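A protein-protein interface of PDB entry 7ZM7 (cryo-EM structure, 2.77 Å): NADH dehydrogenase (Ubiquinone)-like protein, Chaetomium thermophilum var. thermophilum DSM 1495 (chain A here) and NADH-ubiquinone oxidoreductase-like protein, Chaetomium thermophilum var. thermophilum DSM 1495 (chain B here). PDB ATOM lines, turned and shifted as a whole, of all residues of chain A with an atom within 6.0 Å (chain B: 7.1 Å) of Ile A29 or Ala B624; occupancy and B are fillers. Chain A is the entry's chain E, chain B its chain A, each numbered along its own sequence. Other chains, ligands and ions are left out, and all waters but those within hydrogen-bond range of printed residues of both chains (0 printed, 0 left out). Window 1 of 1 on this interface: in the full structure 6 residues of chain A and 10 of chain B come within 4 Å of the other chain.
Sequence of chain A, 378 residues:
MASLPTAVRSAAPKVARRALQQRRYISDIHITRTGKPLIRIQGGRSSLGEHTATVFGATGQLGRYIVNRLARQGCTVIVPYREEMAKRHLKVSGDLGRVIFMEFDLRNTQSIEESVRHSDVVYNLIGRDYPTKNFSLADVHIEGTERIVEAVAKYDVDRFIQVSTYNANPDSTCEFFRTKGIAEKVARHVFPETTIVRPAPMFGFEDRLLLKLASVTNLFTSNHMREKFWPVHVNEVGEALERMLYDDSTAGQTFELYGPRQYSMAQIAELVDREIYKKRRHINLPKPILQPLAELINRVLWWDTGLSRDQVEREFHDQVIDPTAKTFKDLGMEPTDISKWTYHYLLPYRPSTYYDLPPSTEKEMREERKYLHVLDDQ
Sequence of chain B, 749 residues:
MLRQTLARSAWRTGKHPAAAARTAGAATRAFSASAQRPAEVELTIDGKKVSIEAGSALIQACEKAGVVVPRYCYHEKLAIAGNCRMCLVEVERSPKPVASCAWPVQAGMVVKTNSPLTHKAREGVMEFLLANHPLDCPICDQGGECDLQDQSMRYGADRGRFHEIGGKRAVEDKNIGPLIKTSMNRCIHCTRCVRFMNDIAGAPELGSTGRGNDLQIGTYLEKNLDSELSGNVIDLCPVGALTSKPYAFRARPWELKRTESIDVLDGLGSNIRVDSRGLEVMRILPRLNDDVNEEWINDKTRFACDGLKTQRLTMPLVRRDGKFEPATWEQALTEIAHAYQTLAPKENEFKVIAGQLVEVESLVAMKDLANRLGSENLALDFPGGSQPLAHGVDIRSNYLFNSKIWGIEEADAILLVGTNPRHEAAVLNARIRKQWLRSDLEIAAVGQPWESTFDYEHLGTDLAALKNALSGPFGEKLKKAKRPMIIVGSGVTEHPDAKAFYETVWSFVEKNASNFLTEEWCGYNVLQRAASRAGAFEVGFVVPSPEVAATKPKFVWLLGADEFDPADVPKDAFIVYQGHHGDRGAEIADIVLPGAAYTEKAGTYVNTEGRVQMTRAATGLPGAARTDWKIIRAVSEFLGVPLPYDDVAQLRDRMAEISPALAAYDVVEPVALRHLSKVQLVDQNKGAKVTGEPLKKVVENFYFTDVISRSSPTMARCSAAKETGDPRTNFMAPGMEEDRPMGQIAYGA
OD1 of Asp A28 is in salt-bridge range of NH2 of Arg B626 (3.1 Å).
O of Asp A28 lies within hydrogen-bond range of N of Arg A40 (2.9 Å).
The backbone NH (N) of Ala B624 sits at hydrogen-bond distance from the backbone carbonyl oxygen (O) of Thr B314 (2.8 Å).
The backbone carbonyl oxygen of Pro B316 sits at hydrogen-bond distance from the backbone NH of Ala B327, at 2.9 Å.
The backbone carbonyl oxygen of Ser A27 sits at hydrogen-bond distance from the guanidinium group of Arg A40, at 3.2 Å.
The guanidinium group (NH1) of Arg B626 is in hydrogen-bond range of the backbone carbonyl oxygen (O) of Ala B624, at 2.9 Å.
The backbone NH (N) of Arg B626 sits at hydrogen-bond distance from the backbone carbonyl oxygen (O) of Pro B594, at 3.1 Å.
Glu B330 touches Ser A27 (OE1 to OG, 3.6 Å).
OD2 of Asp A28 touches CB of Ala B624, 3.2 Å away.
CD of Pro B316 touches CD1 of Ile A29, at 3.6 Å.
Ala B327 touches Ile A29.
Thr B328 touches Ile A29.
Ile A29 touches Trp B329.
CD1 of Ile A29 touches CB of Ala B624, at 3.8 Å.
Pro A37 touches Met B315.
Gly B623 touches Ile A39 (C to CG2, 3.6 Å).
Ile A39 touches Ala B624.
Printed residues of chain B within 4 Å of Ser A27: Thr B328 (3.96 Å) and Glu B330 (3.6 Å).
Of chain B, only Pro B316 (3.6 Å), Ala B327 (3.9 Å), Thr B328 (3.2 Å), Trp B329 (3.5 Å) and Ala B624 (3.8 Å) come within 4 Å of Ile A29.
Arg A40 touches none of the printed residues of chain B.
Printed residues of chain A within 4 Å of Pro B316: Ile A29.
Printed residues of chain A within 4 Å of Thr B328: Ser A27 and Ile A29.
Of the printed residues of chain A, Trp B329 touches Ile A29 (3.5 Å).
Of the printed residues of chain A, Gly B623 touches Ile A39 (3.6 Å).
Ala B624 touches three residues of chain A.
The nearest residue of chain B that does not touch Ile A29 is Glu B330 (5.2 Å).
Of the 9 printed residues of chain A, 6 touch a printed residue of chain B.
Hydrophobic or aromatic side chains of chain A that line the printed part of chain B: Ile A29, Ile A31, Pro A37 and Ile A39.
Of the 19 printed residues of chain B, 10 touch a printed residue of chain A.
Printed residues of chain B that touch a printed residue of chain A: Met B315, Pro B316, Pro B326, Ala B327, Thr B328, Trp B329, Glu B330, Gly B623, Ala B624 and Arg B626.
Hydrophobic or aromatic side chains of chain B within 4 Å of the printed part of chain A: Met B315, Pro B316, Pro B326, Trp B329 and Ala B624.
Along chain B the printed residues that touch a printed residue of chain A span positions 315 to 626.
Among the printed residues, 13 pairs touch across the chains.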
ATOM      1  N   SER A  27     -33.787  -1.126 -20.267  1.00  0.00           N
ATOM      2  CA  SER A  27     -32.349  -1.185 -20.451  1.00  0.00           C
ATOM      3  C   SER A  27     -32.005  -2.158 -21.572  1.00  0.00           C
ATOM      4  O   SER A  27     -32.784  -3.043 -21.922  1.00  0.00           O
ATOM      5  CB  SER A  27     -31.666  -1.605 -19.153  1.00  0.00           C
ATOM      6  OG  SER A  27     -30.334  -2.019 -19.370  1.00  0.00           O
ATOM      7  N   ASP A  28     -30.824  -1.971 -22.148  1.00  0.00           N
ATOM      8  CA  ASP A  28     -30.389  -2.840 -23.228  1.00  0.00           C
ATOM      9  C   ASP A  28     -29.685  -4.089 -22.735  1.00  0.00           C
ATOM     10  O   ASP A  28     -29.453  -5.002 -23.527  1.00  0.00           O
ATOM     11  CB  ASP A  28     -29.472  -2.076 -24.178  1.00  0.00           C
ATOM     12  CG  ASP A  28     -28.175  -1.672 -23.529  1.00  0.00           C
ATOM     13  OD1 ASP A  28     -28.215  -1.063 -22.443  1.00  0.00           O
ATOM     14  OD2 ASP A  28     -27.114  -1.967 -24.105  1.00  0.00           O
ATOM     15  N   ILE A  29     -29.350  -4.155 -21.457  1.00  0.00           N
ATOM     16  CA  ILE A  29     -28.659  -5.293 -20.877  1.00  0.00           C
ATOM     17  C   ILE A  29     -29.550  -5.875 -19.803  1.00  0.00           C
ATOM     18  O   ILE A  29     -30.104  -5.139 -18.984  1.00  0.00           O
ATOM     19  CB  ILE A  29     -27.298  -4.904 -20.287  1.00  0.00           C
ATOM     20  CG1 ILE A  29     -26.490  -4.088 -21.286  1.00  0.00           C
ATOM     21  CG2 ILE A  29     -26.566  -6.135 -19.840  1.00  0.00           C
ATOM     22  CD1 ILE A  29     -25.579  -3.100 -20.640  1.00  0.00           C
ATOM     23  N   HIS A  30     -29.706  -7.185 -19.820  1.00  0.00           N
ATOM     24  CA  HIS A  30     -30.416  -7.901 -18.779  1.00  0.00           C
ATOM     25  C   HIS A  30     -29.507  -9.012 -18.309  1.00  0.00           C
ATOM     26  O   HIS A  30     -29.096  -9.853 -19.108  1.00  0.00           O
ATOM     27  CB  HIS A  30     -31.734  -8.474 -19.290  1.00  0.00           C
ATOM     28  CG  HIS A  30     -32.488  -9.258 -18.267  1.00  0.00           C
ATOM     29  ND1 HIS A  30     -33.147  -8.662 -17.215  1.00  0.00           N
ATOM     30  CD2 HIS A  30     -32.698 -10.587 -18.142  1.00  0.00           C
ATOM     31  CE1 HIS A  30     -33.723  -9.593 -16.481  1.00  0.00           C
ATOM     32  NE2 HIS A  30     -33.468 -10.770 -17.024  1.00  0.00           N
ATOM     33  N   ILE A  31     -29.170  -8.993 -17.035  1.00  0.00           N
ATOM     34  CA  ILE A  31     -28.507 -10.110 -16.399  1.00  0.00           C
ATOM     35  C   ILE A  31     -29.599 -10.940 -15.759  1.00  0.00           C
ATOM     36  O   ILE A  31     -30.333 -10.449 -14.896  1.00  0.00           O
ATOM     37  CB  ILE A  31     -27.473  -9.644 -15.369  1.00  0.00           C
ATOM     38  CG1 ILE A  31     -26.647  -8.468 -15.917  1.00  0.00           C
ATOM     39  CG2 ILE A  31     -26.577 -10.805 -14.996  1.00  0.00           C
ATOM     40  CD1 ILE A  31     -25.859  -8.775 -17.164  1.00  0.00           C
ATOM     41  N   PRO A  37     -25.841 -12.805 -19.297  1.00  0.00           N
ATOM     42  CA  PRO A  37     -26.264 -11.500 -19.812  1.00  0.00           C
ATOM     43  C   PRO A  37     -26.937 -11.574 -21.173  1.00  0.00           C
ATOM     44  O   PRO A  37     -26.570 -12.361 -22.047  1.00  0.00           O
ATOM     45  CB  PRO A  37     -24.936 -10.742 -19.907  1.00  0.00           C
ATOM     46  CG  PRO A  37     -23.933 -11.790 -20.167  1.00  0.00           C
ATOM     47  CD  PRO A  37     -24.432 -13.088 -19.616  1.00  0.00           C
ATOM     48  N   LEU A  38     -27.929 -10.709 -21.348  1.00  0.00           N
ATOM     49  CA  LEU A  38     -28.652 -10.556 -22.603  1.00  0.00           C
ATOM     50  C   LEU A  38     -28.373  -9.173 -23.162  1.00  0.00           C
ATOM     51  O   LEU A  38     -28.458  -8.185 -22.432  1.00  0.00           O
ATOM     52  CB  LEU A  38     -30.154 -10.730 -22.398  1.00  0.00           C
ATOM     53  CG  LEU A  38     -30.593 -12.040 -21.774  1.00  0.00           C
ATOM     54  CD1 LEU A  38     -32.115 -12.174 -21.832  1.00  0.00           C
ATOM     55  CD2 LEU A  38     -29.909 -13.178 -22.483  1.00  0.00           C
ATOM     56  N   ILE A  39     -28.044  -9.095 -24.447  1.00  0.00           N
ATOM     57  CA  ILE A  39     -27.814  -7.792 -25.061  1.00  0.00           C
ATOM     58  C   ILE A  39     -28.910  -7.551 -26.081  1.00  0.00           C
ATOM     59  O   ILE A  39     -28.780  -7.934 -27.247  1.00  0.00           O
ATOM     60  CB  ILE A  39     -26.436  -7.688 -25.735  1.00  0.00           C
ATOM     61  CG1 ILE A  39     -25.317  -7.854 -24.719  1.00  0.00           C
ATOM     62  CG2 ILE A  39     -26.279  -6.325 -26.343  1.00  0.00           C
ATOM     63  CD1 ILE A  39     -24.890  -9.283 -24.507  1.00  0.00           C
ATOM     64  N   ARG A  40     -29.977  -6.898 -25.665  1.00  0.00           N
ATOM     65  CA  ARG A  40     -31.133  -6.718 -26.518  1.00  0.00           C
ATOM     66  C   ARG A  40     -31.005  -5.468 -27.379  1.00  0.00           C
ATOM     67  O   ARG A  40     -30.376  -4.481 -26.999  1.00  0.00           O
ATOM     68  CB  ARG A  40     -32.404  -6.642 -25.678  1.00  0.00           C
ATOM     69  CG  ARG A  40     -32.654  -5.314 -25.031  1.00  0.00           C
ATOM     70  CD  ARG A  40     -33.847  -5.343 -24.107  1.00  0.00           C
ATOM     71  NE  ARG A  40     -33.542  -5.983 -22.838  1.00  0.00           N
ATOM     72  CZ  ARG A  40     -34.371  -6.030 -21.801  1.00  0.00           C
ATOM     73  NH1 ARG A  40     -34.001  -6.644 -20.693  1.00  0.00           N
ATOM     74  NH2 ARG A  40     -35.561  -5.455 -21.866  1.00  0.00           N
ATOM     75  N   LEU B 313     -14.716  -5.789 -26.064  1.00  0.00           N
ATOM     76  CA  LEU B 313     -15.551  -5.526 -24.902  1.00  0.00           C
ATOM     77  C   LEU B 313     -16.939  -5.155 -25.381  1.00  0.00           C
ATOM     78  O   LEU B 313     -17.105  -4.170 -26.101  1.00  0.00           O
ATOM     79  CB  LEU B 313     -14.970  -4.399 -24.064  1.00  0.00           C
ATOM     80  CG  LEU B 313     -13.468  -4.411 -23.882  1.00  0.00           C
ATOM     81  CD1 LEU B 313     -13.021  -3.139 -23.250  1.00  0.00           C
ATOM     82  CD2 LEU B 313     -13.087  -5.585 -23.052  1.00  0.00           C
ATOM     83  N   THR B 314     -17.935  -5.939 -24.996  1.00  0.00           N
ATOM     84  CA  THR B 314     -19.279  -5.705 -25.476  1.00  0.00           C
ATOM     85  C   THR B 314     -20.294  -5.422 -24.387  1.00  0.00           C
ATOM     86  O   THR B 314     -21.451  -5.155 -24.717  1.00  0.00           O
ATOM     87  CB  THR B 314     -19.760  -6.895 -26.323  1.00  0.00           C
ATOM     88  OG1 THR B 314     -19.782  -8.083 -25.527  1.00  0.00           O
ATOM     89  CG2 THR B 314     -18.855  -7.104 -27.511  1.00  0.00           C
ATOM     90  N   MET B 315     -19.912  -5.461 -23.111  1.00  0.00           N
ATOM     91  CA  MET B 315     -20.847  -5.163 -22.036  1.00  0.00           C
ATOM     92  C   MET B 315     -20.075  -4.667 -20.823  1.00  0.00           C
ATOM     93  O   MET B 315     -18.886  -4.956 -20.696  1.00  0.00           O
ATOM     94  CB  MET B 315     -21.684  -6.396 -21.681  1.00  0.00           C
ATOM     95  CG  MET B 315     -20.891  -7.565 -21.193  1.00  0.00           C
ATOM     96  SD  MET B 315     -21.937  -8.991 -20.928  1.00  0.00           S
ATOM     97  CE  MET B 315     -20.765 -10.314 -21.179  1.00  0.00           C
ATOM     98  N   PRO B 316     -20.707  -3.903 -19.936  1.00  0.00           N
ATOM     99  CA  PRO B 316     -20.002  -3.435 -18.742  1.00  0.00           C
ATOM    100  C   PRO B 316     -19.644  -4.563 -17.790  1.00  0.00           C
ATOM    101  O   PRO B 316     -20.387  -5.526 -17.620  1.00  0.00           O
ATOM    102  CB  PRO B 316     -20.998  -2.463 -18.104  1.00  0.00           C
ATOM    103  CG  PRO B 316     -21.829  -2.024 -19.196  1.00  0.00           C
ATOM    104  CD  PRO B 316     -21.993  -3.213 -20.090  1.00  0.00           C
ATOM    105  N   PRO B 326     -20.594  -9.477 -15.360  1.00  0.00           N
ATOM    106  CA  PRO B 326     -21.387  -8.594 -16.216  1.00  0.00           C
ATOM    107  C   PRO B 326     -22.288  -7.691 -15.402  1.00  0.00           C
ATOM    108  O   PRO B 326     -22.728  -8.039 -14.309  1.00  0.00           O
ATOM    109  CB  PRO B 326     -22.201  -9.566 -17.067  1.00  0.00           C
ATOM    110  CG  PRO B 326     -21.402 -10.763 -17.109  1.00  0.00           C
ATOM    111  CD  PRO B 326     -20.662 -10.872 -15.812  1.00  0.00           C
ATOM    112  N   ALA B 327     -22.558  -6.513 -15.952  1.00  0.00           N
ATOM    113  CA  ALA B 327     -23.403  -5.527 -15.306  1.00  0.00           C
ATOM    114  C   ALA B 327     -24.093  -4.709 -16.383  1.00  0.00           C
ATOM    115  O   ALA B 327     -23.699  -4.733 -17.546  1.00  0.00           O
ATOM    116  CB  ALA B 327     -22.607  -4.616 -14.369  1.00  0.00           C
ATOM    117  N   THR B 328     -25.145  -4.007 -15.988  1.00  0.00           N
ATOM    118  CA  THR B 328     -25.771  -3.030 -16.858  1.00  0.00           C
ATOM    119  C   THR B 328     -25.037  -1.700 -16.777  1.00  0.00           C
ATOM    120  O   THR B 328     -24.124  -1.516 -15.978  1.00  0.00           O
ATOM    121  CB  THR B 328     -27.238  -2.828 -16.502  1.00  0.00           C
ATOM    122  OG1 THR B 328     -27.355  -2.543 -15.112  1.00  0.00           O
ATOM    123  CG2 THR B 328     -28.054  -4.051 -16.846  1.00  0.00           C
ATOM    124  N   TRP B 329     -25.442  -0.769 -17.640  1.00  0.00           N
ATOM    125  CA  TRP B 329     -24.841   0.557 -17.620  1.00  0.00           C
ATOM    126  C   TRP B 329     -25.308   1.350 -16.409  1.00  0.00           C
ATOM    127  O   TRP B 329     -24.503   2.035 -15.775  1.00  0.00           O
ATOM    128  CB  TRP B 329     -25.166   1.308 -18.908  1.00  0.00           C
ATOM    129  CG  TRP B 329     -24.248   1.005 -20.037  1.00  0.00           C
ATOM    130  CD1 TRP B 329     -24.507   0.208 -21.098  1.00  0.00           C
ATOM    131  CD2 TRP B 329     -22.917   1.502 -20.225  1.00  0.00           C
ATOM    132  NE1 TRP B 329     -23.428   0.163 -21.929  1.00  0.00           N
ATOM    133  CE2 TRP B 329     -22.437   0.953 -21.416  1.00  0.00           C
ATOM    134  CE3 TRP B 329     -22.090   2.362 -19.498  1.00  0.00           C
ATOM    135  CZ2 TRP B 329     -21.164   1.230 -21.899  1.00  0.00           C
ATOM    136  CZ3 TRP B 329     -20.838   2.625 -19.969  1.00  0.00           C
ATOM    137  CH2 TRP B 329     -20.380   2.063 -21.154  1.00  0.00           C
ATOM    138  N   GLU B 330     -26.598   1.253 -16.056  1.00  0.00           N
ATOM    139  CA  GLU B 330     -27.111   2.050 -14.945  1.00  0.00           C
ATOM    140  C   GLU B 330     -26.459   1.651 -13.634  1.00  0.00           C
ATOM    141  O   GLU B 330     -26.264   2.493 -12.755  1.00  0.00           O
ATOM    142  CB  GLU B 330     -28.634   1.954 -14.839  1.00  0.00           C
ATOM    143  CG  GLU B 330     -29.195   0.558 -14.570  1.00  0.00           C
ATOM    144  CD  GLU B 330     -29.708  -0.107 -15.827  1.00  0.00           C
ATOM    145  OE1 GLU B 330     -29.424   0.407 -16.927  1.00  0.00           O
ATOM    146  OE2 GLU B 330     -30.398  -1.141 -15.715  1.00  0.00           O
ATOM    147  N   GLN B 331     -26.107   0.383 -13.476  1.00  0.00           N
ATOM    148  CA  GLN B 331     -25.401  -0.049 -12.283  1.00  0.00           C
ATOM    149  C   GLN B 331     -24.011  -0.568 -12.578  1.00  0.00           C
ATOM    150  O   GLN B 331     -23.587  -1.551 -11.981  1.00  0.00           O
ATOM    151  CB  GLN B 331     -26.227  -1.067 -11.495  1.00  0.00           C
ATOM    152  CG  GLN B 331     -26.691  -2.308 -12.212  1.00  0.00           C
ATOM    153  CD  GLN B 331     -25.722  -3.461 -12.177  1.00  0.00           C
ATOM    154  OE1 GLN B 331     -24.927  -3.599 -11.251  1.00  0.00           O
ATOM    155  NE2 GLN B 331     -25.839  -4.346 -13.156  1.00  0.00           N
ATOM    156  N   PRO B 594     -17.176  -0.665 -22.100  1.00  0.00           N
ATOM    157  CA  PRO B 594     -16.876  -0.858 -23.529  1.00  0.00           C
ATOM    158  C   PRO B 594     -17.215   0.354 -24.391  1.00  0.00           C
ATOM    159  O   PRO B 594     -18.373   0.752 -24.502  1.00  0.00           O
ATOM    160  CB  PRO B 594     -17.745  -2.062 -23.898  1.00  0.00           C
ATOM    161  CG  PRO B 594     -18.844  -2.023 -22.938  1.00  0.00           C
ATOM    162  CD  PRO B 594     -18.274  -1.528 -21.659  1.00  0.00           C
ATOM    163  N   GLY B 595     -16.197   0.916 -25.033  1.00  0.00           N
ATOM    164  CA  GLY B 595     -16.365   1.986 -25.989  1.00  0.00           C
ATOM    165  C   GLY B 595     -16.422   1.480 -27.416  1.00  0.00           C
ATOM    166  O   GLY B 595     -16.720   0.313 -27.682  1.00  0.00           O
ATOM    167  N   LEU B 621     -22.037   0.098 -33.476  1.00  0.00           N
ATOM    168  CA  LEU B 621     -21.450  -0.370 -32.230  1.00  0.00           C
ATOM    169  C   LEU B 621     -21.816  -1.830 -31.978  1.00  0.00           C
ATOM    170  O   LEU B 621     -22.963  -2.225 -32.185  1.00  0.00           O
ATOM    171  CB  LEU B 621     -21.947   0.479 -31.061  1.00  0.00           C
ATOM    172  CG  LEU B 621     -21.737   1.992 -31.019  1.00  0.00           C
ATOM    173  CD1 LEU B 621     -22.658   2.615 -30.032  1.00  0.00           C
ATOM    174  CD2 LEU B 621     -20.345   2.284 -30.650  1.00  0.00           C
ATOM    175  N   PRO B 622     -20.873  -2.652 -31.520  1.00  0.00           N
ATOM    176  CA  PRO B 622     -21.194  -4.048 -31.205  1.00  0.00           C
ATOM    177  C   PRO B 622     -21.667  -4.214 -29.767  1.00  0.00           C
ATOM    178  O   PRO B 622     -21.107  -3.624 -28.842  1.00  0.00           O
ATOM    179  CB  PRO B 622     -19.864  -4.770 -31.438  1.00  0.00           C
ATOM    180  CG  PRO B 622     -18.865  -3.768 -31.109  1.00  0.00           C
ATOM    181  CD  PRO B 622     -19.424  -2.428 -31.533  1.00  0.00           C
ATOM    182  N   GLY B 623     -22.695  -5.035 -29.586  1.00  0.00           N
ATOM    183  CA  GLY B 623     -23.190  -5.337 -28.255  1.00  0.00           C
ATOM    184  C   GLY B 623     -23.770  -4.122 -27.580  1.00  0.00           C
ATOM    185  O   GLY B 623     -24.584  -3.399 -28.150  1.00  0.00           O
ATOM    186  N   ALA B 624     -23.360  -3.901 -26.336  1.00  0.00           N
ATOM    187  CA  ALA B 624     -23.808  -2.770 -25.542  1.00  0.00           C
ATOM    188  C   ALA B 624     -22.772  -1.673 -25.457  1.00  0.00           C
ATOM    189  O   ALA B 624     -22.883  -0.805 -24.592  1.00  0.00           O
ATOM    190  CB  ALA B 624     -24.187  -3.222 -24.136  1.00  0.00           C
ATOM    191  N   ALA B 625     -21.763  -1.694 -26.317  1.00  0.00           N
ATOM    192  CA  ALA B 625     -20.768  -0.639 -26.310  1.00  0.00           C
ATOM    193  C   ALA B 625     -21.431   0.708 -26.561  1.00  0.00           C
ATOM    194  O   ALA B 625     -22.566   0.793 -27.026  1.00  0.00           O
ATOM    195  CB  ALA B 625     -19.699  -0.917 -27.363  1.00  0.00           C
ATOM    196  N   ARG B 626     -20.733   1.770 -26.203  1.00  0.00           N
ATOM    197  CA  ARG B 626     -21.256   3.117 -26.318  1.00  0.00           C
ATOM    198  C   ARG B 626     -20.173   4.003 -26.893  1.00  0.00           C
ATOM    199  O   ARG B 626     -18.988   3.704 -26.781  1.00  0.00           O
ATOM    200  CB  ARG B 626     -21.726   3.672 -24.965  1.00  0.00           C
ATOM    201  CG  ARG B 626     -22.898   2.955 -24.357  1.00  0.00           C
ATOM    202  CD  ARG B 626     -24.156   3.296 -25.075  1.00  0.00           C
ATOM    203  NE  ARG B 626     -25.337   2.903 -24.332  1.00  0.00           N
ATOM    204  CZ  ARG B 626     -25.859   1.685 -24.329  1.00  0.00           C
ATOM    205  NH1 ARG B 626     -25.300   0.712 -25.017  1.00  0.00           N
ATOM    206  NH2 ARG B 626     -26.938   1.446 -23.618  1.00  0.00           N
ATOM    207  N   THR B 627     -20.590   5.085 -27.535  1.00  0.00           N
ATOM    208  CA  THR B 627     -19.634   6.062 -28.031  1.00  0.00           C
ATOM    209  C   THR B 627     -18.812   6.616 -26.873  1.00  0.00           C
ATOM    210  O   THR B 627     -19.337   6.875 -25.793  1.00  0.00           O
ATOM    211  CB  THR B 627     -20.364   7.185 -28.755  1.00  0.00           C
ATOM    212  OG1 THR B 627     -21.307   6.624 -29.667  1.00  0.00           O
ATOM    213  CG2 THR B 627     -19.402   8.030 -29.518  1.00  0.00           C
